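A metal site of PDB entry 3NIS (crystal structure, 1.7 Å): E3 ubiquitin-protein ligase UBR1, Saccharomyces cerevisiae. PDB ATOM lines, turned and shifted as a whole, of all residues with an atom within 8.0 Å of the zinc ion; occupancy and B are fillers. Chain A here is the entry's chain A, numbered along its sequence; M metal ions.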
ATOM      1  N   ARG A  23      12.320 -10.053 -26.340  1.00  0.00           N
ATOM      2  CA  ARG A  23      13.160  -9.657 -27.470  1.00  0.00           C
ATOM      3  C   ARG A  23      14.511  -9.202 -26.938  1.00  0.00           C
ATOM      4  O   ARG A  23      14.606  -8.734 -25.800  1.00  0.00           O
ATOM      5  CB  ARG A  23      12.489  -8.584 -28.332  1.00  0.00           C
ATOM      6  CG  ARG A  23      12.227  -7.270 -27.629  1.00  0.00           C
ATOM      7  CD  ARG A  23      11.393  -6.326 -28.480  1.00  0.00           C
ATOM      8  NE  ARG A  23      10.941  -5.189 -27.681  1.00  0.00           N
ATOM      9  CZ  ARG A  23      10.202  -4.179 -28.143  1.00  0.00           C
ATOM     10  NH1 ARG A  23       9.823  -4.150 -29.415  1.00  0.00           N
ATOM     11  NH2 ARG A  23       9.850  -3.201 -27.318  1.00  0.00           N
ATOM     12  N   CYS A  24      15.529  -9.360 -27.764  1.00  0.00           N
ATOM     13  CA  CYS A  24      16.886  -9.000 -27.401  1.00  0.00           C
ATOM     14  C   CYS A  24      17.523  -8.187 -28.522  1.00  0.00           C
ATOM     15  O   CYS A  24      17.638  -8.652 -29.653  1.00  0.00           O
ATOM     16  CB  CYS A  24      17.730 -10.232 -27.106  1.00  0.00           C
ATOM     17  SG  CYS A  24      19.466  -9.822 -26.835  1.00  0.00           S
ATOM     18  N   HIS A  25      17.922  -6.961 -28.194  1.00  0.00           N
ATOM     19  CA  HIS A  25      18.509  -6.052 -29.194  1.00  0.00           C
ATOM     20  C   HIS A  25      19.747  -6.664 -29.881  1.00  0.00           C
ATOM     21  O   HIS A  25      19.912  -6.572 -31.098  1.00  0.00           O
ATOM     22  CB  HIS A  25      18.866  -4.723 -28.543  1.00  0.00           C
ATOM     23  CG  HIS A  25      19.602  -3.782 -29.453  1.00  0.00           C
ATOM     24  ND1 HIS A  25      18.978  -3.107 -30.479  1.00  0.00           N
ATOM     25  CD2 HIS A  25      20.899  -3.404 -29.487  1.00  0.00           C
ATOM     26  CE1 HIS A  25      19.858  -2.356 -31.111  1.00  0.00           C
ATOM     27  NE2 HIS A  25      21.037  -2.507 -30.525  1.00  0.00           N
ATOM     28  N   GLU A  26      20.603  -7.271 -29.088  1.00  0.00           N
ATOM     29  CA  GLU A  26      21.846  -7.840 -29.576  1.00  0.00           C
ATOM     30  C   GLU A  26      21.655  -9.107 -30.403  1.00  0.00           C
ATOM     31  O   GLU A  26      22.302  -9.268 -31.432  1.00  0.00           O
ATOM     32  CB  GLU A  26      22.790  -8.125 -28.407  1.00  0.00           C
ATOM     33  CG  GLU A  26      23.420  -6.859 -27.815  1.00  0.00           C
ATOM     34  CD  GLU A  26      22.524  -6.116 -26.828  1.00  0.00           C
ATOM     35  OE1 GLU A  26      21.407  -6.609 -26.518  1.00  0.00           O
ATOM     36  OE2 GLU A  26      22.937  -5.035 -26.344  1.00  0.00           O
ATOM     37  N   CYS A  27      20.743  -9.975 -29.967  1.00  0.00           N
ATOM     38  CA  CYS A  27      20.622 -11.296 -30.573  1.00  0.00           C
ATOM     39  C   CYS A  27      19.652 -11.342 -31.741  1.00  0.00           C
ATOM     40  O   CYS A  27      19.880 -12.089 -32.694  1.00  0.00           O
ATOM     41  CB  CYS A  27      20.206 -12.358 -29.552  1.00  0.00           C
ATOM     42  SG  CYS A  27      21.475 -12.741 -28.341  1.00  0.00           S
ATOM     43  N   GLY A  28      18.559 -10.581 -31.651  1.00  0.00           N
ATOM     44  CA  GLY A  28      17.513 -10.643 -32.664  1.00  0.00           C
ATOM     45  C   GLY A  28      17.917 -10.054 -34.007  1.00  0.00           C
ATOM     46  O   GLY A  28      18.553  -9.009 -34.063  1.00  0.00           O
ATOM     47  N   LEU A  35      10.981 -14.553 -28.188  1.00  0.00           N
ATOM     48  CA  LEU A  35      11.166 -15.845 -27.529  1.00  0.00           C
ATOM     49  C   LEU A  35      10.122 -16.003 -26.442  1.00  0.00           C
ATOM     50  O   LEU A  35       9.768 -15.028 -25.782  1.00  0.00           O
ATOM     51  CB  LEU A  35      12.554 -15.919 -26.892  1.00  0.00           C
ATOM     52  CG  LEU A  35      13.749 -15.971 -27.839  1.00  0.00           C
ATOM     53  CD1 LEU A  35      15.049 -15.710 -27.070  1.00  0.00           C
ATOM     54  CD2 LEU A  35      13.805 -17.290 -28.584  1.00  0.00           C
ATOM     55  N   PHE A  40      13.303 -18.804 -23.661  1.00  0.00           N
ATOM     56  CA  PHE A  40      14.201 -17.736 -23.267  1.00  0.00           C
ATOM     57  C   PHE A  40      15.154 -18.191 -22.167  1.00  0.00           C
ATOM     58  O   PHE A  40      14.716 -18.610 -21.094  1.00  0.00           O
ATOM     59  CB  PHE A  40      13.408 -16.495 -22.826  1.00  0.00           C
ATOM     60  CG  PHE A  40      14.288 -15.362 -22.397  1.00  0.00           C
ATOM     61  CD1 PHE A  40      14.830 -14.484 -23.340  1.00  0.00           C
ATOM     62  CD2 PHE A  40      14.601 -15.171 -21.040  1.00  0.00           C
ATOM     63  CE1 PHE A  40      15.630 -13.445 -22.952  1.00  0.00           C
ATOM     64  CE2 PHE A  40      15.419 -14.118 -20.634  1.00  0.00           C
ATOM     65  CZ  PHE A  40      15.944 -13.254 -21.596  1.00  0.00           C
ATOM     66  N   ASN A  41      16.451 -18.120 -22.459  1.00  0.00           N
ATOM     67  CA  ASN A  41      17.491 -18.526 -21.538  1.00  0.00           C
ATOM     68  C   ASN A  41      18.248 -17.278 -21.079  1.00  0.00           C
ATOM     69  O   ASN A  41      19.025 -16.707 -21.843  1.00  0.00           O
ATOM     70  CB  ASN A  41      18.444 -19.519 -22.227  1.00  0.00           C
ATOM     71  CG  ASN A  41      19.435 -20.148 -21.266  1.00  0.00           C
ATOM     72  OD1 ASN A  41      19.654 -19.651 -20.169  1.00  0.00           O
ATOM     73  ND2 ASN A  41      20.065 -21.247 -21.692  1.00  0.00           N
ATOM     74  N   PRO A  42      18.001 -16.844 -19.828  1.00  0.00           N
ATOM     75  CA  PRO A  42      18.630 -15.654 -19.267  1.00  0.00           C
ATOM     76  C   PRO A  42      20.151 -15.656 -19.438  1.00  0.00           C
ATOM     77  O   PRO A  42      20.750 -14.592 -19.632  1.00  0.00           O
ATOM     78  CB  PRO A  42      18.264 -15.734 -17.782  1.00  0.00           C
ATOM     79  CG  PRO A  42      16.945 -16.438 -17.789  1.00  0.00           C
ATOM     80  CD  PRO A  42      17.075 -17.479 -18.858  1.00  0.00           C
ATOM     81  N   LYS A  43      20.748 -16.845 -19.398  1.00  0.00           N
ATOM     82  CA  LYS A  43      22.196 -16.992 -19.544  1.00  0.00           C
ATOM     83  C   LYS A  43      22.724 -16.547 -20.906  1.00  0.00           C
ATOM     84  O   LYS A  43      23.873 -16.117 -21.005  1.00  0.00           O
ATOM     85  CB  LYS A  43      22.624 -18.428 -19.271  1.00  0.00           C
ATOM     86  CG  LYS A  43      22.496 -18.828 -17.815  1.00  0.00           C
ATOM     87  CD  LYS A  43      23.122 -20.196 -17.550  1.00  0.00           C
ATOM     88  CE  LYS A  43      22.119 -21.304 -17.788  1.00  0.00           C
ATOM     89  NZ  LYS A  43      22.601 -22.641 -17.341  1.00  0.00           N
ATOM     90  N   ASP A  44      21.898 -16.666 -21.953  1.00  0.00           N
ATOM     91  CA  ASP A  44      22.270 -16.187 -23.291  1.00  0.00           C
ATOM     92  C   ASP A  44      22.347 -14.651 -23.365  1.00  0.00           C
ATOM     93  O   ASP A  44      22.982 -14.119 -24.277  1.00  0.00           O
ATOM     94  CB  ASP A  44      21.268 -16.655 -24.347  1.00  0.00           C
ATOM     95  CG  ASP A  44      21.413 -18.124 -24.701  1.00  0.00           C
ATOM     96  OD1 ASP A  44      22.499 -18.715 -24.463  1.00  0.00           O
ATOM     97  OD2 ASP A  44      20.423 -18.691 -25.238  1.00  0.00           O
ATOM     98  N   HIS A  45      21.721 -13.967 -22.416  1.00  0.00           N
ATOM     99  CA  HIS A  45      21.432 -12.539 -22.569  1.00  0.00           C
ATOM    100  C   HIS A  45      21.857 -11.662 -21.392  1.00  0.00           C
ATOM    101  O   HIS A  45      21.355 -10.545 -21.231  1.00  0.00           O
ATOM    102  CB  HIS A  45      19.939 -12.369 -22.861  1.00  0.00           C
ATOM    103  CG  HIS A  45      19.427 -13.270 -23.956  1.00  0.00           C
ATOM    104  ND1 HIS A  45      19.737 -13.076 -25.284  1.00  0.00           N
ATOM    105  CD2 HIS A  45      18.645 -14.376 -23.915  1.00  0.00           C
ATOM    106  CE1 HIS A  45      19.168 -14.015 -26.010  1.00  0.00           C
ATOM    107  NE2 HIS A  45      18.505 -14.823 -25.205  1.00  0.00           N
ATOM    108  N   VAL A  46      22.795 -12.164 -20.593  1.00  0.00           N
ATOM    109  CA  VAL A  46      23.209 -11.539 -19.333  1.00  0.00           C
ATOM    110  C   VAL A  46      23.473 -10.020 -19.441  1.00  0.00           C
ATOM    111  O   VAL A  46      22.955  -9.240 -18.627  1.00  0.00           O
ATOM    112  CB  VAL A  46      24.447 -12.273 -18.725  1.00  0.00           C
ATOM    113  CG1 VAL A  46      24.998 -11.509 -17.527  1.00  0.00           C
ATOM    114  CG2 VAL A  46      24.060 -13.688 -18.294  1.00  0.00           C
ATOM    115  N   ASN A  47      24.285  -9.623 -20.408  1.00  0.00           N
ATOM    116  CA  ASN A  47      24.584  -8.192 -20.595  1.00  0.00           C
ATOM    117  C   ASN A  47      23.996  -7.644 -21.876  1.00  0.00           C
ATOM    118  O   ASN A  47      24.571  -6.779 -22.546  1.00  0.00           O
ATOM    119  CB  ASN A  47      26.096  -7.926 -20.492  1.00  0.00           C
ATOM    120  CG  ASN A  47      26.923  -8.995 -21.167  1.00  0.00           C
ATOM    121  OD1 ASN A  47      26.467  -9.643 -22.119  1.00  0.00           O
ATOM    122  ND2 ASN A  47      28.135  -9.197 -20.677  1.00  0.00           N
ATOM    123  N   HIS A  48      22.823  -8.168 -22.234  1.00  0.00           N
ATOM    124  CA  HIS A  48      22.123  -7.739 -23.426  1.00  0.00           C
ATOM    125  C   HIS A  48      20.948  -6.861 -23.030  1.00  0.00           C
ATOM    126  O   HIS A  48      20.494  -6.890 -21.884  1.00  0.00           O
ATOM    127  CB  HIS A  48      21.653  -8.962 -24.219  1.00  0.00           C
ATOM    128  CG  HIS A  48      22.773  -9.765 -24.811  1.00  0.00           C
ATOM    129  ND1 HIS A  48      22.549 -10.833 -25.661  1.00  0.00           N
ATOM    130  CD2 HIS A  48      24.115  -9.649 -24.707  1.00  0.00           C
ATOM    131  CE1 HIS A  48      23.705 -11.344 -26.029  1.00  0.00           C
ATOM    132  NE2 HIS A  48      24.672 -10.647 -25.457  1.00  0.00           N
ATOM    133  N   HIS A  49      20.460  -6.083 -23.988  1.00  0.00           N
ATOM    134  CA  HIS A  49      19.279  -5.248 -23.791  1.00  0.00           C
ATOM    135  C   HIS A  49      18.025  -6.011 -24.178  1.00  0.00           C
ATOM    136  O   HIS A  49      17.617  -6.032 -25.337  1.00  0.00           O
ATOM    137  CB  HIS A  49      19.401  -3.943 -24.590  1.00  0.00           C
ATOM    138  CG  HIS A  49      20.543  -3.080 -24.160  1.00  0.00           C
ATOM    139  ND1 HIS A  49      21.850  -3.353 -24.499  1.00  0.00           N
ATOM    140  CD2 HIS A  49      20.571  -1.947 -23.407  1.00  0.00           C
ATOM    141  CE1 HIS A  49      22.633  -2.423 -23.975  1.00  0.00           C
ATOM    142  NE2 HIS A  49      21.884  -1.560 -23.317  1.00  0.00           N
ATOM    143  N   VAL A  50      17.430  -6.664 -23.177  1.00  0.00           N
ATOM    144  CA  VAL A  50      16.238  -7.488 -23.350  1.00  0.00           C
ATOM    145  C   VAL A  50      14.996  -6.705 -22.930  1.00  0.00           C
ATOM    146  O   VAL A  50      15.007  -6.002 -21.915  1.00  0.00           O
ATOM    147  CB  VAL A  50      16.350  -8.823 -22.553  1.00  0.00           C
ATOM    148  CG1 VAL A  50      15.042  -9.629 -22.593  1.00  0.00           C
ATOM    149  CG2 VAL A  50      17.497  -9.659 -23.090  1.00  0.00           C
ATOM    150  N   TRP A  71      17.973 -15.021 -35.471  1.00  0.00           N
ATOM    151  CA  TRP A  71      19.003 -14.776 -34.438  1.00  0.00           C
ATOM    152  C   TRP A  71      20.416 -14.652 -34.998  1.00  0.00           C
ATOM    153  O   TRP A  71      20.819 -15.412 -35.886  1.00  0.00           O
ATOM    154  CB  TRP A  71      18.947 -15.878 -33.365  1.00  0.00           C
ATOM    155  CG  TRP A  71      17.545 -16.051 -32.867  1.00  0.00           C
ATOM    156  CD1 TRP A  71      16.694 -17.090 -33.160  1.00  0.00           C
ATOM    157  CD2 TRP A  71      16.806 -15.148 -32.046  1.00  0.00           C
ATOM    158  NE1 TRP A  71      15.475 -16.881 -32.562  1.00  0.00           N
ATOM    159  CE2 TRP A  71      15.516 -15.705 -31.868  1.00  0.00           C
ATOM    160  CE3 TRP A  71      17.115 -13.926 -31.433  1.00  0.00           C
ATOM    161  CZ2 TRP A  71      14.540 -15.065 -31.108  1.00  0.00           C
ATOM    162  CZ3 TRP A  71      16.140 -13.299 -30.676  1.00  0.00           C
ATOM    163  CH2 TRP A  71      14.864 -13.874 -30.520  1.00  0.00           C
ATOM    164  N   SER A  73      23.128 -14.816 -32.924  1.00  0.00           N
ATOM    165  CA  SER A  73      23.966 -15.659 -32.075  1.00  0.00           C
ATOM    166  C   SER A  73      23.266 -16.991 -31.802  1.00  0.00           C
ATOM    167  O   SER A  73      22.026 -17.078 -31.835  1.00  0.00           O
ATOM    168  CB  SER A  73      24.275 -14.944 -30.751  1.00  0.00           C
ATOM    169  OG  SER A  73      24.894 -13.689 -30.977  1.00  0.00           O
ATOM    170  N   PRO A  74      24.062 -18.051 -31.548  1.00  0.00           N
ATOM    171  CA  PRO A  74      23.446 -19.345 -31.227  1.00  0.00           C
ATOM    172  C   PRO A  74      22.672 -19.233 -29.923  1.00  0.00           C
ATOM    173  O   PRO A  74      23.203 -18.720 -28.930  1.00  0.00           O
ATOM    174  CB  PRO A  74      24.658 -20.279 -31.081  1.00  0.00           C
ATOM    175  CG  PRO A  74      25.821 -19.379 -30.780  1.00  0.00           C
ATOM    176  CD  PRO A  74      25.538 -18.113 -31.538  1.00  0.00           C
ATOM    177  N   LEU A  75      21.401 -19.625 -29.939  1.00  0.00           N
ATOM    178  CA  LEU A  75      20.597 -19.656 -28.720  1.00  0.00           C
ATOM    179  C   LEU A  75      20.705 -21.019 -28.055  1.00  0.00           C
ATOM    180  O   LEU A  75      20.851 -22.039 -28.727  1.00  0.00           O
ATOM    181  CB  LEU A  75      19.120 -19.322 -28.999  1.00  0.00           C
ATOM    182  CG  LEU A  75      18.729 -17.957 -29.569  1.00  0.00           C
ATOM    183  CD1 LEU A  75      17.231 -17.787 -29.540  1.00  0.00           C
ATOM    184  CD2 LEU A  75      19.391 -16.806 -28.816  1.00  0.00           C
HETATM  185 ZN    ZN M   1      20.733 -11.607 -26.441  1.00  0.00          ZN
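The side-chain sulfur of Cys 24 lies close to the backbone NH of Glu 26 (3.6 Å).
The zinc ion is bound by a ring nitrogen (ND1) of His 45 (2.1 Å), a ring nitrogen (ND1) of His 48 (2.1 Å), the side-chain sulfur of Cys 24 (2.2 Å) and the side-chain sulfur of Cys 27 (2.3 Å).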
